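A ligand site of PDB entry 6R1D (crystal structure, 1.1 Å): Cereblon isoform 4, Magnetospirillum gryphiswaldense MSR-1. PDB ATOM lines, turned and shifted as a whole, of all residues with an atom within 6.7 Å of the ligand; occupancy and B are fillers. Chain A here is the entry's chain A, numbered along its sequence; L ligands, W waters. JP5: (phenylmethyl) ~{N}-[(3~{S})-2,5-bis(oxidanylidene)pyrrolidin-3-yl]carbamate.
The indole nitrogen (NE1) of Trp 100 sits close to a nitrogen (N) of the ligand, 3.4 Å away.
Merely in contact with the ligand: Pro 52 (3.6 Å), Glu 77 (3.97 Å), Ser 79 (3.5 Å), Trp 86 (3.4 Å), Ile 88 (3.5 Å) and His 97 (3.4 Å).
Hydrophobic or aromatic side chains that line the ligand: Pro 52, Trp 80, Trp 86, Ile 88, His 97, Trp 100 and Tyr 102.
The side-chain amide oxygen (OD1) of Asn 51 lies within hydrogen-bond range of the backbone NH (N) of Met 55 (2.9 Å).
O of Phe 50 sits at hydrogen-bond distance from NE1 of Trp 80.
The backbone carbonyl oxygen of Glu 77 sits at hydrogen-bond distance from the indole nitrogen of Trp 86.
N of Trp 86 is in hydrogen-bond range of O of Ser 75 (2.8 Å).
NE2 of His 97 is in hydrogen-bond range of O of Gly 99 (3.0 Å).
The backbone carbonyl oxygen of His 97 lies within hydrogen-bond range of the guanidinium group of Arg 118 (2.9 Å).
The side-chain hydroxyl of Ser 79 sits at hydrogen-bond distance from the backbone carbonyl oxygen of Tyr 84.
N of Glu 77 is in hydrogen-bond range of OG of Ser 75 (3.0 Å).
OH of Tyr 102 lies within hydrogen-bond range of OD1 of the ligand, 2.8 Å away.
O of Phe 78 lies within hydrogen-bond range of ND2 of the ligand (2.8 Å).
An oxygen (OAK) of the ligand lies within hydrogen-bond range of the side-chain amide nitrogen (ND2) of Asn 51.
An oxygen (OD1) of the ligand sits at hydrogen-bond distance from the backbone NH of Trp 80 (3.0 Å).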
ATOM      1  N   PHE A  50      12.223 -33.047  -1.199  1.00  0.00           N
ATOM      2  CA  PHE A  50      11.822 -32.951   0.163  1.00  0.00           C
ATOM      3  C   PHE A  50      13.025 -32.559   0.995  1.00  0.00           C
ATOM      4  O   PHE A  50      14.166 -32.840   0.644  1.00  0.00           O
ATOM      5  CB  PHE A  50      11.151 -34.222   0.710  1.00  0.00           C
ATOM      6  CG  PHE A  50      11.988 -35.484   0.690  1.00  0.00           C
ATOM      7  CD1 PHE A  50      12.863 -35.791   1.644  1.00  0.00           C
ATOM      8  CD2 PHE A  50      11.839 -36.349  -0.330  1.00  0.00           C
ATOM      9  CE1 PHE A  50      13.595 -37.031   1.552  1.00  0.00           C
ATOM     10  CE2 PHE A  50      12.482 -37.561  -0.383  1.00  0.00           C
ATOM     11  CZ  PHE A  50      13.338 -37.874   0.598  1.00  0.00           C
ATOM     12  N   ASN A  51      12.747 -31.907   2.130  1.00  0.00           N
ATOM     13  CA  ASN A  51      13.814 -31.562   3.044  1.00  0.00           C
ATOM     14  C   ASN A  51      13.953 -32.697   4.149  1.00  0.00           C
ATOM     15  O   ASN A  51      13.152 -33.614   4.136  1.00  0.00           O
ATOM     16  CB  ASN A  51      13.648 -30.176   3.631  1.00  0.00           C
ATOM     17  CG  ASN A  51      12.530 -30.000   4.572  1.00  0.00           C
ATOM     18  OD1 ASN A  51      11.920 -30.971   5.033  1.00  0.00           O
ATOM     19  ND2 ASN A  51      12.131 -28.724   4.834  1.00  0.00           N
ATOM     20  N   PRO A  52      14.972 -32.621   4.964  1.00  0.00           N
ATOM     21  CA  PRO A  52      15.163 -33.740   5.901  1.00  0.00           C
ATOM     22  C   PRO A  52      14.077 -33.917   6.819  1.00  0.00           C
ATOM     23  O   PRO A  52      13.867 -35.023   7.358  1.00  0.00           O
ATOM     24  CB  PRO A  52      16.486 -33.310   6.614  1.00  0.00           C
ATOM     25  CG  PRO A  52      17.203 -32.599   5.565  1.00  0.00           C
ATOM     26  CD  PRO A  52      16.170 -31.772   4.943  1.00  0.00           C
ATOM     27  N   MET A  55       9.276 -32.181   4.575  1.00  0.00           N
ATOM     28  CA  MET A  55       8.439 -31.245   3.867  1.00  0.00           C
ATOM     29  C   MET A  55       8.699 -31.394   2.371  1.00  0.00           C
ATOM     30  O   MET A  55       9.869 -31.398   1.972  1.00  0.00           O
ATOM     31  CB  MET A  55       8.719 -29.844   4.376  1.00  0.00           C
ATOM     32  CG  MET A  55       8.561 -29.715   5.857  1.00  0.00           C
ATOM     33  SD  MET A  55       9.150 -28.211   6.654  1.00  0.00           S
ATOM     34  CE  MET A  55       7.948 -27.175   6.071  1.00  0.00           C
ATOM     35  N   PHE A  57       8.265 -30.182  -1.640  1.00  0.00           N
ATOM     36  CA  PHE A  57       8.167 -28.974  -2.467  1.00  0.00           C
ATOM     37  C   PHE A  57       8.323 -29.284  -3.889  1.00  0.00           C
ATOM     38  O   PHE A  57       9.161 -30.086  -4.286  1.00  0.00           O
ATOM     39  CB  PHE A  57       9.244 -27.972  -2.055  1.00  0.00           C
ATOM     40  CG  PHE A  57       9.285 -27.591  -0.614  1.00  0.00           C
ATOM     41  CD1 PHE A  57       8.570 -26.522  -0.092  1.00  0.00           C
ATOM     42  CD2 PHE A  57      10.157 -28.263   0.265  1.00  0.00           C
ATOM     43  CE1 PHE A  57       8.649 -26.171   1.207  1.00  0.00           C
ATOM     44  CE2 PHE A  57      10.223 -27.931   1.575  1.00  0.00           C
ATOM     45  CZ  PHE A  57       9.445 -26.851   2.062  1.00  0.00           C
ATOM     46  N   ILE A  71      16.766 -14.466   4.135  1.00  0.00           N
ATOM     47  CA  ILE A  71      16.977 -14.514   5.606  1.00  0.00           C
ATOM     48  C   ILE A  71      17.929 -15.606   5.967  1.00  0.00           C
ATOM     49  O   ILE A  71      17.978 -16.642   5.308  1.00  0.00           O
ATOM     50  CB  ILE A  71      15.631 -14.609   6.322  1.00  0.00           C
ATOM     51  CG1 ILE A  71      14.900 -15.899   6.002  1.00  0.00           C
ATOM     52  CG2 ILE A  71      14.789 -13.378   6.067  1.00  0.00           C
ATOM     53  CD1 ILE A  71      13.708 -16.158   6.880  1.00  0.00           C
ATOM     54  N   SER A  75      23.512 -22.106   3.657  1.00  0.00           N
ATOM     55  CA  SER A  75      23.693 -23.425   4.158  1.00  0.00           C
ATOM     56  C   SER A  75      23.944 -24.380   3.002  1.00  0.00           C
ATOM     57  O   SER A  75      23.216 -24.374   2.011  1.00  0.00           O
ATOM     58  CB  SER A  75      22.592 -23.908   4.985  1.00  0.00           C
ATOM     59  OG  SER A  75      22.775 -25.196   5.438  1.00  0.00           O
ATOM     60  N   GLY A  76      24.841 -25.336   3.197  1.00  0.00           N
ATOM     61  CA  GLY A  76      24.952 -26.431   2.260  1.00  0.00           C
ATOM     62  C   GLY A  76      24.150 -27.679   2.650  1.00  0.00           C
ATOM     63  O   GLY A  76      24.159 -28.683   1.907  1.00  0.00           O
ATOM     64  N   GLU A  77      23.480 -27.633   3.780  1.00  0.00           N
ATOM     65  CA  GLU A  77      22.834 -28.803   4.315  1.00  0.00           C
ATOM     66  C   GLU A  77      21.732 -29.352   3.411  1.00  0.00           C
ATOM     67  O   GLU A  77      20.832 -28.669   3.047  1.00  0.00           O
ATOM     68  CB  GLU A  77      22.208 -28.465   5.647  1.00  0.00           C
ATOM     69  CG  GLU A  77      21.521 -29.669   6.357  1.00  0.00           C
ATOM     70  CD  GLU A  77      21.029 -29.344   7.801  1.00  0.00           C
ATOM     71  OE1 GLU A  77      21.425 -28.267   8.311  1.00  0.00           O
ATOM     72  OE2 GLU A  77      20.252 -30.176   8.446  1.00  0.00           O
ATOM     73  N   PHE A  78      21.963 -30.635   2.953  1.00  0.00           N
ATOM     74  CA  PHE A  78      20.979 -31.312   2.148  1.00  0.00           C
ATOM     75  C   PHE A  78      20.603 -30.471   0.949  1.00  0.00           C
ATOM     76  O   PHE A  78      19.451 -30.461   0.491  1.00  0.00           O
ATOM     77  CB  PHE A  78      19.771 -31.734   2.894  1.00  0.00           C
ATOM     78  CG  PHE A  78      19.055 -32.927   2.365  1.00  0.00           C
ATOM     79  CD1 PHE A  78      19.671 -34.168   2.373  1.00  0.00           C
ATOM     80  CD2 PHE A  78      17.773 -32.899   1.913  1.00  0.00           C
ATOM     81  CE1 PHE A  78      19.004 -35.262   1.958  1.00  0.00           C
ATOM     82  CE2 PHE A  78      17.068 -33.974   1.449  1.00  0.00           C
ATOM     83  CZ  PHE A  78      17.696 -35.193   1.510  1.00  0.00           C
ATOM     84  N   SER A  79      21.561 -29.798   0.346  1.00  0.00           N
ATOM     85  CA  SER A  79      21.218 -28.952  -0.790  1.00  0.00           C
ATOM     86  C   SER A  79      20.729 -29.794  -1.941  1.00  0.00           C
ATOM     87  O   SER A  79      21.326 -30.802  -2.311  1.00  0.00           O
ATOM     88  CB  SER A  79      22.421 -28.164  -1.270  1.00  0.00           C
ATOM     89  OG  SER A  79      21.974 -27.347  -2.337  1.00  0.00           O
ATOM     90  N   TRP A  80      19.616 -29.379  -2.514  1.00  0.00           N
ATOM     91  CA  TRP A  80      19.042 -30.093  -3.635  1.00  0.00           C
ATOM     92  C   TRP A  80      19.866 -29.904  -4.924  1.00  0.00           C
ATOM     93  O   TRP A  80      19.639 -30.642  -5.868  1.00  0.00           O
ATOM     94  CB  TRP A  80      17.602 -29.659  -3.849  1.00  0.00           C
ATOM     95  CG  TRP A  80      16.734 -29.994  -2.705  1.00  0.00           C
ATOM     96  CD1 TRP A  80      16.669 -31.192  -2.000  1.00  0.00           C
ATOM     97  CD2 TRP A  80      15.737 -29.146  -2.124  1.00  0.00           C
ATOM     98  NE1 TRP A  80      15.759 -31.105  -1.024  1.00  0.00           N
ATOM     99  CE2 TRP A  80      15.134 -29.862  -1.068  1.00  0.00           C
ATOM    100  CE3 TRP A  80      15.321 -27.815  -2.353  1.00  0.00           C
ATOM    101  CZ2 TRP A  80      14.139 -29.348  -0.286  1.00  0.00           C
ATOM    102  CZ3 TRP A  80      14.345 -27.319  -1.561  1.00  0.00           C
ATOM    103  CH2 TRP A  80      13.745 -28.044  -0.545  1.00  0.00           C
ATOM    104  N   PHE A  81      20.790 -28.940  -4.944  1.00  0.00           N
ATOM    105  CA  PHE A  81      21.555 -28.664  -6.110  1.00  0.00           C
ATOM    106  C   PHE A  81      22.984 -28.733  -5.676  1.00  0.00           C
ATOM    107  O   PHE A  81      23.544 -27.863  -5.056  1.00  0.00           O
ATOM    108  CB  PHE A  81      21.208 -27.291  -6.669  1.00  0.00           C
ATOM    109  CG  PHE A  81      19.735 -27.189  -7.040  1.00  0.00           C
ATOM    110  CD1 PHE A  81      19.303 -27.782  -8.181  1.00  0.00           C
ATOM    111  CD2 PHE A  81      18.830 -26.599  -6.201  1.00  0.00           C
ATOM    112  CE1 PHE A  81      17.927 -27.732  -8.476  1.00  0.00           C
ATOM    113  CE2 PHE A  81      17.514 -26.556  -6.484  1.00  0.00           C
ATOM    114  CZ  PHE A  81      17.057 -27.168  -7.576  1.00  0.00           C
ATOM    115  N   TYR A  84      25.845 -26.012  -4.580  1.00  0.00           N
ATOM    116  CA  TYR A  84      25.266 -24.724  -4.284  1.00  0.00           C
ATOM    117  C   TYR A  84      24.769 -24.713  -2.829  1.00  0.00           C
ATOM    118  O   TYR A  84      24.233 -25.694  -2.330  1.00  0.00           O
ATOM    119  CB  TYR A  84      24.088 -24.441  -5.175  1.00  0.00           C
ATOM    120  CG  TYR A  84      24.476 -24.200  -6.634  1.00  0.00           C
ATOM    121  CD1 TYR A  84      24.701 -22.899  -7.081  1.00  0.00           C
ATOM    122  CD2 TYR A  84      24.668 -25.222  -7.483  1.00  0.00           C
ATOM    123  CE1 TYR A  84      25.129 -22.678  -8.361  1.00  0.00           C
ATOM    124  CE2 TYR A  84      25.123 -24.956  -8.796  1.00  0.00           C
ATOM    125  CZ  TYR A  84      25.368 -23.695  -9.195  1.00  0.00           C
ATOM    126  OH  TYR A  84      25.835 -23.507 -10.487  1.00  0.00           O
ATOM    127  N   TRP A  86      22.221 -22.708  -0.014  1.00  0.00           N
ATOM    128  CA  TRP A  86      20.947 -22.057  -0.057  1.00  0.00           C
ATOM    129  C   TRP A  86      20.742 -21.065   1.075  1.00  0.00           C
ATOM    130  O   TRP A  86      21.224 -21.272   2.208  1.00  0.00           O
ATOM    131  CB  TRP A  86      19.801 -23.080  -0.046  1.00  0.00           C
ATOM    132  CG  TRP A  86      19.883 -24.109   1.039  1.00  0.00           C
ATOM    133  CD1 TRP A  86      20.407 -25.372   0.913  1.00  0.00           C
ATOM    134  CD2 TRP A  86      19.378 -24.034   2.371  1.00  0.00           C
ATOM    135  NE1 TRP A  86      20.249 -26.028   2.043  1.00  0.00           N
ATOM    136  CE2 TRP A  86      19.605 -25.258   2.965  1.00  0.00           C
ATOM    137  CE3 TRP A  86      18.690 -23.051   3.103  1.00  0.00           C
ATOM    138  CZ2 TRP A  86      19.248 -25.517   4.299  1.00  0.00           C
ATOM    139  CZ3 TRP A  86      18.281 -23.306   4.365  1.00  0.00           C
ATOM    140  CH2 TRP A  86      18.585 -24.543   4.988  1.00  0.00           C
ATOM    141  N   ILE A  88      17.130 -18.996   2.643  1.00  0.00           N
ATOM    142  CA  ILE A  88      15.690 -18.888   2.530  1.00  0.00           C
ATOM    143  C   ILE A  88      15.236 -17.572   1.958  1.00  0.00           C
ATOM    144  O   ILE A  88      15.790 -16.528   2.345  1.00  0.00           O
ATOM    145  CB  ILE A  88      15.138 -19.080   3.956  1.00  0.00           C
ATOM    146  CG1 ILE A  88      15.444 -20.451   4.479  1.00  0.00           C
ATOM    147  CG2 ILE A  88      13.588 -18.822   3.978  1.00  0.00           C
ATOM    148  CD1 ILE A  88      15.454 -20.509   6.023  1.00  0.00           C
ATOM    149  N   HIS A  97       6.760 -17.768   2.386  1.00  0.00           N
ATOM    150  CA  HIS A  97       7.982 -18.475   2.045  1.00  0.00           C
ATOM    151  C   HIS A  97       7.913 -18.878   0.600  1.00  0.00           C
ATOM    152  O   HIS A  97       7.159 -19.779   0.233  1.00  0.00           O
ATOM    153  CB  HIS A  97       8.165 -19.670   2.964  1.00  0.00           C
ATOM    154  CG  HIS A  97       9.346 -20.524   2.565  1.00  0.00           C
ATOM    155  ND1 HIS A  97       9.314 -21.887   2.659  1.00  0.00           N
ATOM    156  CD2 HIS A  97      10.532 -20.163   2.008  1.00  0.00           C
ATOM    157  CE1 HIS A  97      10.495 -22.313   2.159  1.00  0.00           C
ATOM    158  NE2 HIS A  97      11.234 -21.301   1.776  1.00  0.00           N
ATOM    159  N   GLY A  99      10.713 -19.657  -1.430  1.00  0.00           N
ATOM    160  CA  GLY A  99      11.742 -20.651  -1.840  1.00  0.00           C
ATOM    161  C   GLY A  99      13.069 -20.309  -1.247  1.00  0.00           C
ATOM    162  O   GLY A  99      13.180 -20.023  -0.063  1.00  0.00           O
ATOM    163  N   TRP A 100      14.084 -20.411  -2.119  1.00  0.00           N
ATOM    164  CA  TRP A 100      15.466 -20.296  -1.728  1.00  0.00           C
ATOM    165  C   TRP A 100      16.256 -19.593  -2.772  1.00  0.00           C
ATOM    166  O   TRP A 100      15.989 -19.713  -3.979  1.00  0.00           O
ATOM    167  CB  TRP A 100      16.109 -21.685  -1.464  1.00  0.00           C
ATOM    168  CG  TRP A 100      15.445 -22.474  -0.360  1.00  0.00           C
ATOM    169  CD1 TRP A 100      15.860 -22.505   0.929  1.00  0.00           C
ATOM    170  CD2 TRP A 100      14.286 -23.273  -0.444  1.00  0.00           C
ATOM    171  NE1 TRP A 100      15.019 -23.289   1.660  1.00  0.00           N
ATOM    172  CE2 TRP A 100      14.021 -23.775   0.843  1.00  0.00           C
ATOM    173  CE3 TRP A 100      13.408 -23.594  -1.460  1.00  0.00           C
ATOM    174  CZ2 TRP A 100      12.998 -24.610   1.135  1.00  0.00           C
ATOM    175  CZ3 TRP A 100      12.313 -24.432  -1.170  1.00  0.00           C
ATOM    176  CH2 TRP A 100      12.100 -24.903   0.107  1.00  0.00           C
ATOM    177  N   TYR A 102      20.184 -19.699  -4.217  1.00  0.00           N
ATOM    178  CA  TYR A 102      21.349 -20.574  -4.294  1.00  0.00           C
ATOM    179  C   TYR A 102      22.521 -19.813  -4.800  1.00  0.00           C
ATOM    180  O   TYR A 102      22.466 -19.052  -5.755  1.00  0.00           O
ATOM    181  CB  TYR A 102      21.021 -21.786  -5.237  1.00  0.00           C
ATOM    182  CG  TYR A 102      20.082 -22.720  -4.615  1.00  0.00           C
ATOM    183  CD1 TYR A 102      20.445 -23.770  -3.806  1.00  0.00           C
ATOM    184  CD2 TYR A 102      18.700 -22.576  -4.855  1.00  0.00           C
ATOM    185  CE1 TYR A 102      19.547 -24.607  -3.212  1.00  0.00           C
ATOM    186  CE2 TYR A 102      17.787 -23.400  -4.248  1.00  0.00           C
ATOM    187  CZ  TYR A 102      18.209 -24.428  -3.435  1.00  0.00           C
ATOM    188  OH  TYR A 102      17.282 -25.228  -2.859  1.00  0.00           O
ATOM    189  N   ARG A 118       3.438 -21.641  -4.653  1.00  0.00           N
ATOM    190  CA  ARG A 118       3.356 -20.385  -3.923  1.00  0.00           C
ATOM    191  C   ARG A 118       3.405 -19.163  -4.887  1.00  0.00           C
ATOM    192  O   ARG A 118       3.398 -18.047  -4.382  1.00  0.00           O
ATOM    193  CB  ARG A 118       4.470 -20.266  -2.924  1.00  0.00           C
ATOM    194  CG  ARG A 118       4.431 -21.358  -1.834  1.00  0.00           C
ATOM    195  CD  ARG A 118       4.180 -20.983  -0.567  1.00  0.00           C
ATOM    196  NE  ARG A 118       3.984 -22.206   0.229  1.00  0.00           N
ATOM    197  CZ  ARG A 118       4.808 -22.715   1.111  1.00  0.00           C
ATOM    198  NH1 ARG A 118       5.930 -22.162   1.386  1.00  0.00           N
ATOM    199  NH2 ARG A 118       4.424 -23.814   1.795  1.00  0.00           N
HETATM  200  O   JP5 L   1      16.721 -29.065   2.705  1.00  0.00           O
HETATM  201  C   JP5 L   1      16.844 -28.195   1.852  1.00  0.00           C
HETATM  202  ND2 JP5 L   1      17.615 -28.348   0.736  1.00  0.00           N
HETATM  203  CG  JP5 L   1      17.662 -27.214  -0.027  1.00  0.00           C
HETATM  204  OD1 JP5 L   1      18.244 -27.108  -1.058  1.00  0.00           O
HETATM  205  CB  JP5 L   1      16.843 -26.115   0.648  1.00  0.00           C
HETATM  206  CA  JP5 L   1      16.157 -26.877   1.782  1.00  0.00           C
HETATM  207  N   JP5 L   1      16.126 -26.206   3.062  1.00  0.00           N
HETATM  208  CAI JP5 L   1      15.161 -26.339   3.883  1.00  0.00           C
HETATM  209  OAK JP5 L   1      14.077 -26.921   3.659  1.00  0.00           O
HETATM  210  OAJ JP5 L   1      15.404 -25.777   5.096  1.00  0.00           O
HETATM  211  CAL JP5 L   1      14.417 -25.740   6.131  1.00  0.00           C
HETATM  212  CAM JP5 L   1      13.348 -24.761   5.874  1.00  0.00           C
HETATM  213  CAN JP5 L   1      12.040 -25.208   5.783  1.00  0.00           C
HETATM  214  CAO JP5 L   1      11.065 -24.395   5.550  1.00  0.00           C
HETATM  215  CAP JP5 L   1      11.150 -22.973   5.439  1.00  0.00           C
HETATM  216  CAQ JP5 L   1      12.506 -22.554   5.585  1.00  0.00           C
HETATM  217  CAR JP5 L   1      13.523 -23.421   5.704  1.00  0.00           C
HETATM  218  O   HOH W   1       8.058 -23.769   4.505  1.00  0.00           O
HETATM  219  O   HOH W   2      16.602 -28.391   5.818  1.00  0.00           O
